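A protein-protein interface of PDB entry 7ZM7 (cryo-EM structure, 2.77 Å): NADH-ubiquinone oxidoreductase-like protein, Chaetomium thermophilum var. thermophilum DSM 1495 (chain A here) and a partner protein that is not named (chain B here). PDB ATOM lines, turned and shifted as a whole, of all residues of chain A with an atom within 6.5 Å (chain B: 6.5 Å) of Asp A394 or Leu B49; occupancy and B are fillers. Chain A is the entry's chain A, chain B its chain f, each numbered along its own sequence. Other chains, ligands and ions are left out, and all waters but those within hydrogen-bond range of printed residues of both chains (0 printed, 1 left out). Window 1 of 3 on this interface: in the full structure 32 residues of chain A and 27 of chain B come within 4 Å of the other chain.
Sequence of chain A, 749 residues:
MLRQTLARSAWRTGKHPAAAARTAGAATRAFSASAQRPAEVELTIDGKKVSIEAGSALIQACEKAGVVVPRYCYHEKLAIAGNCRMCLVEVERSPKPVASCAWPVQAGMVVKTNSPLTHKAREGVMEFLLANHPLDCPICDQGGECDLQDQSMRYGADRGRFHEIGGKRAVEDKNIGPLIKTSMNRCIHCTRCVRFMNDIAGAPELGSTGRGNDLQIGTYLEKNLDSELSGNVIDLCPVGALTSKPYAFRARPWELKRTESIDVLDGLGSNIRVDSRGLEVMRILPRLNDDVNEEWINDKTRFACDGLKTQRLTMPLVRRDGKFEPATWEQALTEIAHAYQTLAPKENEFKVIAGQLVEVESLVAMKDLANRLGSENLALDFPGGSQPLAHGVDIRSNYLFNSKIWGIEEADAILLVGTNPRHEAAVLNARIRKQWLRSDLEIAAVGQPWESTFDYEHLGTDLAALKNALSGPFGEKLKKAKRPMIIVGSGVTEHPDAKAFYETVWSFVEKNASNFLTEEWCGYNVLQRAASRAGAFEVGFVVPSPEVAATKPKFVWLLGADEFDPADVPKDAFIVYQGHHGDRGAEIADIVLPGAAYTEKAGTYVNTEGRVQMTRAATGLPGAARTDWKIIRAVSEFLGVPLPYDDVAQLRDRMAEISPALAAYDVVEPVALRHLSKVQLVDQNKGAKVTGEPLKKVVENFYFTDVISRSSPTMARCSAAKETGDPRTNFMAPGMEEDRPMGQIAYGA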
ATOM      1  N   LYS A 367      24.612 -21.020  19.044  1.00  0.00           N
ATOM      2  CA  LYS A 367      23.569 -20.605  18.118  1.00  0.00           C
ATOM      3  C   LYS A 367      22.198 -20.869  18.702  1.00  0.00           C
ATOM      4  O   LYS A 367      21.300 -20.029  18.601  1.00  0.00           O
ATOM      5  CB  LYS A 367      23.707 -21.323  16.783  1.00  0.00           C
ATOM      6  CG  LYS A 367      23.087 -20.562  15.637  1.00  0.00           C
ATOM      7  CD  LYS A 367      22.652 -21.464  14.510  1.00  0.00           C
ATOM      8  CE  LYS A 367      22.255 -20.649  13.299  1.00  0.00           C
ATOM      9  NZ  LYS A 367      21.870 -21.496  12.156  1.00  0.00           N
ATOM     10  N   GLY A 392      27.348 -14.903   0.430  1.00  0.00           N
ATOM     11  CA  GLY A 392      26.321 -15.394   1.317  1.00  0.00           C
ATOM     12  C   GLY A 392      26.795 -16.621   2.062  1.00  0.00           C
ATOM     13  O   GLY A 392      27.985 -16.937   2.113  1.00  0.00           O
ATOM     14  N   VAL A 393      25.841 -17.320   2.660  1.00  0.00           N
ATOM     15  CA  VAL A 393      26.130 -18.634   3.208  1.00  0.00           C
ATOM     16  C   VAL A 393      25.062 -19.611   2.739  1.00  0.00           C
ATOM     17  O   VAL A 393      24.903 -20.693   3.303  1.00  0.00           O
ATOM     18  CB  VAL A 393      26.228 -18.598   4.742  1.00  0.00           C
ATOM     19  CG1 VAL A 393      27.498 -17.923   5.162  1.00  0.00           C
ATOM     20  CG2 VAL A 393      25.046 -17.896   5.333  1.00  0.00           C
ATOM     21  N   ASP A 394      24.346 -19.246   1.686  1.00  0.00           N
ATOM     22  CA  ASP A 394      23.199 -20.040   1.259  1.00  0.00           C
ATOM     23  C   ASP A 394      23.627 -21.237   0.428  1.00  0.00           C
ATOM     24  O   ASP A 394      23.174 -22.360   0.665  1.00  0.00           O
ATOM     25  CB  ASP A 394      22.238 -19.150   0.493  1.00  0.00           C
ATOM     26  CG  ASP A 394      21.810 -17.970   1.309  1.00  0.00           C
ATOM     27  OD1 ASP A 394      21.860 -18.077   2.551  1.00  0.00           O
ATOM     28  OD2 ASP A 394      21.440 -16.933   0.726  1.00  0.00           O
ATOM     29  N   ILE A 395      24.497 -21.014  -0.550  1.00  0.00           N
ATOM     30  CA  ILE A 395      25.170 -22.074  -1.281  1.00  0.00           C
ATOM     31  C   ILE A 395      26.513 -22.299  -0.610  1.00  0.00           C
ATOM     32  O   ILE A 395      27.202 -21.335  -0.268  1.00  0.00           O
ATOM     33  CB  ILE A 395      25.355 -21.705  -2.764  1.00  0.00           C
ATOM     34  CG1 ILE A 395      24.054 -21.187  -3.375  1.00  0.00           C
ATOM     35  CG2 ILE A 395      25.857 -22.877  -3.537  1.00  0.00           C
ATOM     36  CD1 ILE A 395      22.890 -22.112  -3.236  1.00  0.00           C
ATOM     37  N   ARG A 396      26.902 -23.560  -0.436  1.00  0.00           N
ATOM     38  CA  ARG A 396      28.196 -23.861   0.225  1.00  0.00           C
ATOM     39  C   ARG A 396      29.329 -23.364  -0.665  1.00  0.00           C
ATOM     40  O   ARG A 396      30.347 -22.932  -0.116  1.00  0.00           O
ATOM     41  CB  ARG A 396      28.327 -25.336   0.609  1.00  0.00           C
ATOM     42  CG  ARG A 396      27.479 -25.736   1.806  1.00  0.00           C
ATOM     43  CD  ARG A 396      27.403 -27.237   1.992  1.00  0.00           C
ATOM     44  NE  ARG A 396      28.700 -27.865   2.183  1.00  0.00           N
ATOM     45  CZ  ARG A 396      29.193 -28.814   1.399  1.00  0.00           C
ATOM     46  NH1 ARG A 396      30.385 -29.326   1.651  1.00  0.00           N
ATOM     47  NH2 ARG A 396      28.489 -29.254   0.371  1.00  0.00           N
ATOM     48  N   SER A 397      29.136 -23.370  -1.980  1.00  0.00           N
ATOM     49  CA  SER A 397      30.205 -22.993  -2.887  1.00  0.00           C
ATOM     50  C   SER A 397      30.495 -21.501  -2.873  1.00  0.00           C
ATOM     51  O   SER A 397      31.493 -21.082  -3.468  1.00  0.00           O
ATOM     52  CB  SER A 397      29.854 -23.461  -4.299  1.00  0.00           C
ATOM     53  OG  SER A 397      28.939 -22.588  -4.907  1.00  0.00           O
ATOM     54  N   ASN A 398      29.664 -20.697  -2.203  1.00  0.00           N
ATOM     55  CA  ASN A 398      29.876 -19.254  -2.161  1.00  0.00           C
ATOM     56  C   ASN A 398      31.160 -18.896  -1.439  1.00  0.00           C
ATOM     57  O   ASN A 398      31.863 -17.963  -1.837  1.00  0.00           O
ATOM     58  CB  ASN A 398      28.704 -18.564  -1.476  1.00  0.00           C
ATOM     59  CG  ASN A 398      27.454 -18.618  -2.287  1.00  0.00           C
ATOM     60  OD1 ASN A 398      27.420 -19.260  -3.323  1.00  0.00           O
ATOM     61  ND2 ASN A 398      26.408 -17.962  -1.817  1.00  0.00           N
ATOM     62  N   TYR A 399      31.472 -19.624  -0.361  1.00  0.00           N
ATOM     63  CA  TYR A 399      32.563 -19.189   0.544  1.00  0.00           C
ATOM     64  C   TYR A 399      33.674 -20.219   0.651  1.00  0.00           C
ATOM     65  O   TYR A 399      34.535 -20.060   1.533  1.00  0.00           O
ATOM     66  CB  TYR A 399      32.004 -18.995   1.952  1.00  0.00           C
ATOM     67  CG  TYR A 399      31.122 -20.109   2.463  1.00  0.00           C
ATOM     68  CD1 TYR A 399      31.665 -21.253   3.024  1.00  0.00           C
ATOM     69  CD2 TYR A 399      29.743 -20.007   2.414  1.00  0.00           C
ATOM     70  CE1 TYR A 399      30.863 -22.277   3.501  1.00  0.00           C
ATOM     71  CE2 TYR A 399      28.927 -21.021   2.886  1.00  0.00           C
ATOM     72  CZ  TYR A 399      29.488 -22.159   3.435  1.00  0.00           C
ATOM     73  OH  TYR A 399      28.691 -23.160   3.904  1.00  0.00           O
ATOM     74  N   PHE A 537      30.163 -20.513   8.766  1.00  0.00           N
ATOM     75  CA  PHE A 537      29.370 -20.305   7.533  1.00  0.00           C
ATOM     76  C   PHE A 537      28.511 -21.538   7.294  1.00  0.00           C
ATOM     77  O   PHE A 537      27.360 -21.382   6.870  1.00  0.00           O
ATOM     78  CB  PHE A 537      30.325 -20.056   6.368  1.00  0.00           C
ATOM     79  CG  PHE A 537      31.234 -18.860   6.497  1.00  0.00           C
ATOM     80  CD1 PHE A 537      30.950 -17.833   7.381  1.00  0.00           C
ATOM     81  CD2 PHE A 537      32.379 -18.762   5.724  1.00  0.00           C
ATOM     82  CE1 PHE A 537      31.800 -16.746   7.502  1.00  0.00           C
ATOM     83  CE2 PHE A 537      33.224 -17.671   5.841  1.00  0.00           C
ATOM     84  CZ  PHE A 537      32.933 -16.664   6.728  1.00  0.00           C
ATOM     85  N   GLU A 538      29.057 -22.720   7.560  1.00  0.00           N
ATOM     86  CA  GLU A 538      28.342 -23.994   7.317  1.00  0.00           C
ATOM     87  C   GLU A 538      27.084 -24.083   8.193  1.00  0.00           C
ATOM     88  O   GLU A 538      26.063 -24.566   7.692  1.00  0.00           O
ATOM     89  CB  GLU A 538      29.333 -25.142   7.524  1.00  0.00           C
ATOM     90  CG  GLU A 538      28.812 -26.500   7.104  1.00  0.00           C
ATOM     91  CD  GLU A 538      28.833 -26.785   5.613  1.00  0.00           C
ATOM     92  OE1 GLU A 538      29.235 -25.894   4.838  1.00  0.00           O
ATOM     93  OE2 GLU A 538      28.459 -27.907   5.227  1.00  0.00           O
ATOM     94  N   VAL A 539      27.158 -23.651   9.450  1.00  0.00           N
ATOM     95  CA  VAL A 539      25.995 -23.725  10.387  1.00  0.00           C
ATOM     96  C   VAL A 539      25.179 -22.432  10.336  1.00  0.00           C
ATOM     97  O   VAL A 539      24.189 -22.366  11.055  1.00  0.00           O
ATOM     98  CB  VAL A 539      26.420 -24.106  11.819  1.00  0.00           C
ATOM     99  CG1 VAL A 539      27.112 -25.454  11.849  1.00  0.00           C
ATOM    100  CG2 VAL A 539      27.287 -23.040  12.469  1.00  0.00           C
ATOM    101  N   GLY A 540      25.569 -21.465   9.506  1.00  0.00           N
ATOM    102  CA  GLY A 540      24.806 -20.212   9.333  1.00  0.00           C
ATOM    103  C   GLY A 540      24.988 -19.240  10.473  1.00  0.00           C
ATOM    104  O   GLY A 540      24.086 -18.432  10.698  1.00  0.00           O
ATOM    105  N   ILE A 658      21.579 -29.279  10.973  1.00  0.00           N
ATOM    106  CA  ILE A 658      21.912 -27.986  10.313  1.00  0.00           C
ATOM    107  C   ILE A 658      22.613 -28.246   8.983  1.00  0.00           C
ATOM    108  O   ILE A 658      22.228 -27.630   7.982  1.00  0.00           O
ATOM    109  CB  ILE A 658      22.779 -27.116  11.237  1.00  0.00           C
ATOM    110  CG1 ILE A 658      22.022 -26.725  12.507  1.00  0.00           C
ATOM    111  CG2 ILE A 658      23.287 -25.896  10.495  1.00  0.00           C
ATOM    112  CD1 ILE A 658      22.749 -27.057  13.777  1.00  0.00           C
ATOM    113  N   VAL A 679      23.078 -15.978  -7.282  1.00  0.00           N
ATOM    114  CA  VAL A 679      22.035 -15.171  -6.670  1.00  0.00           C
ATOM    115  C   VAL A 679      22.561 -14.413  -5.458  1.00  0.00           C
ATOM    116  O   VAL A 679      22.103 -13.307  -5.170  1.00  0.00           O
ATOM    117  CB  VAL A 679      20.825 -16.045  -6.323  1.00  0.00           C
ATOM    118  CG1 VAL A 679      20.402 -16.830  -7.546  1.00  0.00           C
ATOM    119  CG2 VAL A 679      21.156 -16.937  -5.212  1.00  0.00           C
ATOM    120  N   GLN A 680      23.522 -14.977  -4.726  1.00  0.00           N
ATOM    121  CA  GLN A 680      24.150 -14.189  -3.668  1.00  0.00           C
ATOM    122  C   GLN A 680      25.261 -13.305  -4.196  1.00  0.00           C
ATOM    123  O   GLN A 680      25.349 -12.133  -3.824  1.00  0.00           O
ATOM    124  CB  GLN A 680      24.715 -15.082  -2.573  1.00  0.00           C
ATOM    125  CG  GLN A 680      23.686 -15.853  -1.842  1.00  0.00           C
ATOM    126  CD  GLN A 680      22.797 -14.943  -1.061  1.00  0.00           C
ATOM    127  OE1 GLN A 680      23.245 -13.962  -0.481  1.00  0.00           O
ATOM    128  NE2 GLN A 680      21.514 -15.233  -1.076  1.00  0.00           N
ATOM    129  N   GLU B  13      14.689 -18.789   9.228  1.00  0.00           N
ATOM    130  CA  GLU B  13      15.704 -19.462   8.432  1.00  0.00           C
ATOM    131  C   GLU B  13      15.130 -20.747   7.871  1.00  0.00           C
ATOM    132  O   GLU B  13      14.504 -21.514   8.603  1.00  0.00           O
ATOM    133  CB  GLU B  13      16.947 -19.750   9.289  1.00  0.00           C
ATOM    134  CG  GLU B  13      17.904 -20.788   8.748  1.00  0.00           C
ATOM    135  CD  GLU B  13      19.066 -21.008   9.696  1.00  0.00           C
ATOM    136  OE1 GLU B  13      19.758 -22.040   9.582  1.00  0.00           O
ATOM    137  OE2 GLU B  13      19.283 -20.145  10.571  1.00  0.00           O
ATOM    138  N   LEU B  14      15.355 -20.976   6.584  1.00  0.00           N
ATOM    139  CA  LEU B  14      14.968 -22.201   5.896  1.00  0.00           C
ATOM    140  C   LEU B  14      16.194 -23.050   5.628  1.00  0.00           C
ATOM    141  O   LEU B  14      17.266 -22.522   5.335  1.00  0.00           O
ATOM    142  CB  LEU B  14      14.284 -21.908   4.569  1.00  0.00           C
ATOM    143  CG  LEU B  14      12.872 -21.383   4.598  1.00  0.00           C
ATOM    144  CD1 LEU B  14      12.434 -21.428   3.174  1.00  0.00           C
ATOM    145  CD2 LEU B  14      12.015 -22.277   5.460  1.00  0.00           C
ATOM    146  N   ARG B  15      16.026 -24.358   5.793  1.00  0.00           N
ATOM    147  CA  ARG B  15      17.191 -25.257   5.660  1.00  0.00           C
ATOM    148  C   ARG B  15      16.776 -26.505   4.897  1.00  0.00           C
ATOM    149  O   ARG B  15      16.059 -27.330   5.458  1.00  0.00           O
ATOM    150  CB  ARG B  15      17.706 -25.659   7.043  1.00  0.00           C
ATOM    151  CG  ARG B  15      19.185 -25.386   7.264  1.00  0.00           C
ATOM    152  CD  ARG B  15      19.422 -25.347   8.757  1.00  0.00           C
ATOM    153  NE  ARG B  15      18.944 -26.559   9.398  1.00  0.00           N
ATOM    154  CZ  ARG B  15      18.640 -26.654  10.685  1.00  0.00           C
ATOM    155  NH1 ARG B  15      18.222 -27.805  11.180  1.00  0.00           N
ATOM    156  NH2 ARG B  15      18.743 -25.598  11.470  1.00  0.00           N
ATOM    157  N   PHE B  16      17.222 -26.621   3.657  1.00  0.00           N
ATOM    158  CA  PHE B  16      16.965 -27.784   2.820  1.00  0.00           C
ATOM    159  C   PHE B  16      18.135 -28.737   2.945  1.00  0.00           C
ATOM    160  O   PHE B  16      19.287 -28.327   2.799  1.00  0.00           O
ATOM    161  CB  PHE B  16      16.772 -27.383   1.360  1.00  0.00           C
ATOM    162  CG  PHE B  16      15.586 -26.507   1.133  1.00  0.00           C
ATOM    163  CD1 PHE B  16      15.697 -25.135   1.232  1.00  0.00           C
ATOM    164  CD2 PHE B  16      14.354 -27.046   0.841  1.00  0.00           C
ATOM    165  CE1 PHE B  16      14.615 -24.336   1.026  1.00  0.00           C
ATOM    166  CE2 PHE B  16      13.276 -26.239   0.641  1.00  0.00           C
ATOM    167  CZ  PHE B  16      13.408 -24.894   0.740  1.00  0.00           C
ATOM    168  N   LEU B  17      17.835 -29.980   3.308  1.00  0.00           N
ATOM    169  CA  LEU B  17      18.876 -31.032   3.401  1.00  0.00           C
ATOM    170  C   LEU B  17      18.580 -32.077   2.329  1.00  0.00           C
ATOM    171  O   LEU B  17      17.469 -32.606   2.352  1.00  0.00           O
ATOM    172  CB  LEU B  17      18.814 -31.677   4.783  1.00  0.00           C
ATOM    173  CG  LEU B  17      18.899 -30.759   5.998  1.00  0.00           C
ATOM    174  CD1 LEU B  17      19.122 -31.601   7.239  1.00  0.00           C
ATOM    175  CD2 LEU B  17      20.013 -29.738   5.852  1.00  0.00           C
ATOM    176  N   PHE B  18      19.519 -32.357   1.427  1.00  0.00           N
ATOM    177  CA  PHE B  18      19.284 -33.285   0.322  1.00  0.00           C
ATOM    178  C   PHE B  18      20.606 -33.904  -0.104  1.00  0.00           C
ATOM    179  O   PHE B  18      21.641 -33.690   0.524  1.00  0.00           O
ATOM    180  CB  PHE B  18      18.560 -32.559  -0.812  1.00  0.00           C
ATOM    181  CG  PHE B  18      19.325 -31.430  -1.378  1.00  0.00           C
ATOM    182  CD1 PHE B  18      19.254 -30.188  -0.792  1.00  0.00           C
ATOM    183  CD2 PHE B  18      20.054 -31.574  -2.526  1.00  0.00           C
ATOM    184  CE1 PHE B  18      19.944 -29.133  -1.309  1.00  0.00           C
ATOM    185  CE2 PHE B  18      20.735 -30.510  -3.050  1.00  0.00           C
ATOM    186  CZ  PHE B  18      20.676 -29.296  -2.444  1.00  0.00           C
ATOM    187  N   TYR B  36      14.530 -21.510  -5.432  1.00  0.00           N
ATOM    188  CA  TYR B  36      15.351 -20.737  -4.506  1.00  0.00           C
ATOM    189  C   TYR B  36      15.738 -19.345  -5.003  1.00  0.00           C
ATOM    190  O   TYR B  36      15.657 -18.399  -4.202  1.00  0.00           O
ATOM    191  CB  TYR B  36      16.591 -21.567  -4.146  1.00  0.00           C
ATOM    192  CG  TYR B  36      17.753 -20.740  -3.714  1.00  0.00           C
ATOM    193  CD1 TYR B  36      17.835 -20.253  -2.429  1.00  0.00           C
ATOM    194  CD2 TYR B  36      18.756 -20.429  -4.590  1.00  0.00           C
ATOM    195  CE1 TYR B  36      18.875 -19.488  -2.041  1.00  0.00           C
ATOM    196  CE2 TYR B  36      19.795 -19.670  -4.207  1.00  0.00           C
ATOM    197  CZ  TYR B  36      19.857 -19.195  -2.933  1.00  0.00           C
ATOM    198  OH  TYR B  36      20.918 -18.423  -2.538  1.00  0.00           O
ATOM    199  N   LYS B  40      14.678 -16.061  -2.908  1.00  0.00           N
ATOM    200  CA  LYS B  40      15.688 -15.178  -2.267  1.00  0.00           C
ATOM    201  C   LYS B  40      15.487 -13.758  -2.783  1.00  0.00           C
ATOM    202  O   LYS B  40      15.790 -12.810  -2.044  1.00  0.00           O
ATOM    203  CB  LYS B  40      17.098 -15.707  -2.558  1.00  0.00           C
ATOM    204  CG  LYS B  40      18.270 -14.800  -2.191  1.00  0.00           C
ATOM    205  CD  LYS B  40      18.315 -14.322  -0.749  1.00  0.00           C
ATOM    206  CE  LYS B  40      18.167 -15.408   0.295  1.00  0.00           C
ATOM    207  NZ  LYS B  40      18.915 -16.638  -0.051  1.00  0.00           N
ATOM    208  N   ILE B  46      16.409 -13.073   4.938  1.00  0.00           N
ATOM    209  CA  ILE B  46      16.322 -14.382   5.574  1.00  0.00           C
ATOM    210  C   ILE B  46      17.383 -15.280   4.953  1.00  0.00           C
ATOM    211  O   ILE B  46      17.516 -15.311   3.723  1.00  0.00           O
ATOM    212  CB  ILE B  46      14.926 -15.003   5.425  1.00  0.00           C
ATOM    213  CG1 ILE B  46      13.873 -14.153   6.125  1.00  0.00           C
ATOM    214  CG2 ILE B  46      14.906 -16.392   6.016  1.00  0.00           C
ATOM    215  CD1 ILE B  46      13.259 -13.088   5.255  1.00  0.00           C
ATOM    216  N   PRO B  47      18.163 -16.007   5.750  1.00  0.00           N
ATOM    217  CA  PRO B  47      19.024 -17.046   5.186  1.00  0.00           C
ATOM    218  C   PRO B  47      18.207 -18.233   4.705  1.00  0.00           C
ATOM    219  O   PRO B  47      17.263 -18.667   5.365  1.00  0.00           O
ATOM    220  CB  PRO B  47      19.910 -17.434   6.373  1.00  0.00           C
ATOM    221  CG  PRO B  47      19.033 -17.179   7.552  1.00  0.00           C
ATOM    222  CD  PRO B  47      18.299 -15.925   7.213  1.00  0.00           C
ATOM    223  N   ILE B  48      18.585 -18.771   3.553  1.00  0.00           N
ATOM    224  CA  ILE B  48      17.944 -19.962   2.990  1.00  0.00           C
ATOM    225  C   ILE B  48      19.070 -20.938   2.670  1.00  0.00           C
ATOM    226  O   ILE B  48      19.633 -20.919   1.574  1.00  0.00           O
ATOM    227  CB  ILE B  48      17.108 -19.653   1.747  1.00  0.00           C
ATOM    228  CG1 ILE B  48      16.129 -18.521   2.024  1.00  0.00           C
ATOM    229  CG2 ILE B  48      16.348 -20.854   1.329  1.00  0.00           C
ATOM    230  CD1 ILE B  48      15.592 -17.875   0.809  1.00  0.00           C
ATOM    231  N   LEU B  49      19.402 -21.801   3.620  1.00  0.00           N
ATOM    232  CA  LEU B  49      20.610 -22.597   3.524  1.00  0.00           C
ATOM    233  C   LEU B  49      20.326 -23.916   2.831  1.00  0.00           C
ATOM    234  O   LEU B  49      19.417 -24.652   3.219  1.00  0.00           O
ATOM    235  CB  LEU B  49      21.216 -22.858   4.898  1.00  0.00           C
ATOM    236  CG  LEU B  49      21.379 -21.660   5.817  1.00  0.00           C
ATOM    237  CD1 LEU B  49      21.665 -22.178   7.191  1.00  0.00           C
ATOM    238  CD2 LEU B  49      22.458 -20.700   5.338  1.00  0.00           C
ATOM    239  N   LEU B  50      21.111 -24.205   1.805  1.00  0.00           N
ATOM    240  CA  LEU B  50      21.026 -25.458   1.084  1.00  0.00           C
ATOM    241  C   LEU B  50      22.257 -26.249   1.485  1.00  0.00           C
ATOM    242  O   LEU B  50      23.380 -25.878   1.137  1.00  0.00           O
ATOM    243  CB  LEU B  50      20.971 -25.220  -0.420  1.00  0.00           C
ATOM    244  CG  LEU B  50      20.021 -24.149  -0.944  1.00  0.00           C
ATOM    245  CD1 LEU B  50      20.018 -24.188  -2.438  1.00  0.00           C
ATOM    246  CD2 LEU B  50      18.660 -24.374  -0.439  1.00  0.00           C
ATOM    247  N   ARG B  51      22.030 -27.297   2.275  1.00  0.00           N
ATOM    248  CA  ARG B  51      23.139 -28.132   2.783  1.00  0.00           C
ATOM    249  C   ARG B  51      22.884 -29.584   2.377  1.00  0.00           C
ATOM    250  O   ARG B  51      21.854 -30.122   2.770  1.00  0.00           O
ATOM    251  CB  ARG B  51      23.280 -27.933   4.294  1.00  0.00           C
ATOM    252  CG  ARG B  51      23.537 -26.500   4.729  1.00  0.00           C
ATOM    253  CD  ARG B  51      24.967 -26.113   4.440  1.00  0.00           C
ATOM    254  NE  ARG B  51      25.285 -24.835   5.044  1.00  0.00           N
ATOM    255  CZ  ARG B  51      25.201 -23.668   4.427  1.00  0.00           C
ATOM    256  NH1 ARG B  51      25.505 -22.560   5.077  1.00  0.00           N
ATOM    257  NH2 ARG B  51      24.818 -23.611   3.166  1.00  0.00           N
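The guanidinium group (NE) of Arg B51 sits at hydrogen-bond distance from the backbone carbonyl oxygen (O) of Glu A538 (2.8 Å). NH1 of Arg B51 lies within hydrogen-bond range of O of Val A393 (2.6 Å). The backbone carbonyl oxygen (O) of Asp A394 lies within hydrogen-bond range of the backbone NH (N) of Leu B50, 3.0 Å away. The guanidinium group of Arg B51 is in hydrogen-bond range of the backbone carbonyl oxygen of Asp A394 (3.2 Å). NE2 of Gln A680 lies close to NZ of Lys B40 (3.1 Å). OE2 of Glu B13 lies within salt-bridge range of NZ of Lys A367, 3.3 Å away. NH1 of Arg B51 sits at hydrogen-bond distance from O of Phe A537 (2.8 Å). The guanidinium group of Arg B51 is in hydrogen-bond range of the side-chain hydroxyl of Tyr A399 (3.4 Å). OD2 of Asp A394 lies within salt-bridge range of NZ of Lys B40 (2.7 Å). The backbone NH (N) of Ile B48 lies within hydrogen-bond range of the side-chain carboxylate (OD1) of Asp A394 (3.5 Å).
The side-chain amino group of Lys A367 sits at hydrogen-bond distance from the backbone carbonyl oxygen of Val A539, at 2.7 Å. O of Phe B16 is in hydrogen-bond range of N of Arg B51 (3.0 Å). The guanidinium group (NE) of Arg A396 is in salt-bridge range of the side-chain carboxylate (OE2) of Glu A538 (3.1 Å). OE1 of Glu A538 sits at hydrogen-bond distance from OH of Tyr A399 (2.9 Å). The backbone NH (N) of Phe B16 lies within hydrogen-bond range of the backbone carbonyl oxygen (O) of Leu B49 (3.0 Å). The side-chain carboxylate (OD2) of Asp A394 sits at hydrogen-bond distance from the side-chain amide nitrogen (NE2) of Gln A680 (2.5 Å).
Among the printed residues, pairs that only touch across the chains: Val A679 with Tyr B36, Val A393 with Leu B49, Asp A394 with Tyr B36, Ile A658 with Arg B15, Gln A680 with Tyr B36, Arg A396 with Arg B51, Ile A395 with Leu B50, Ile A658 with Arg B51, Ile A658 with Leu B17 and Asp A394 with Leu B49.
Of the printed residues of chain B, Asp A394 touches Tyr B36 (3.4 Å), Lys B40 (2.7 Å), Ile B48 (3.3 Å), Leu B49 (3.8 Å), Leu B50 (3.0 Å) and Arg B51 (3.2 Å). Printed residues of chain B within 4 Å of Arg A396: Arg B51 (3.6 Å). Of the printed residues of chain B, Val A679 touches Tyr B36 (3.1 Å). Leu B49 touches just these residues of chain A: Val A393 and Asp A394. The nearest printed residue of chain B that does not touch Ile A395 is Tyr B36 (4.1 Å).
Hydrophobic or aromatic side chains of chain B that line the printed part of chain A: Leu B17, Tyr B36, Leu B49 and Leu B50. Among the printed residues, Asp or Glu carboxylates within 4 Å of a Lys or Arg side-chain nitrogen of the other chain: Lys A367 with Glu B13 (3.3 Å) and Asp A394 with Lys B40 (2.7 Å).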
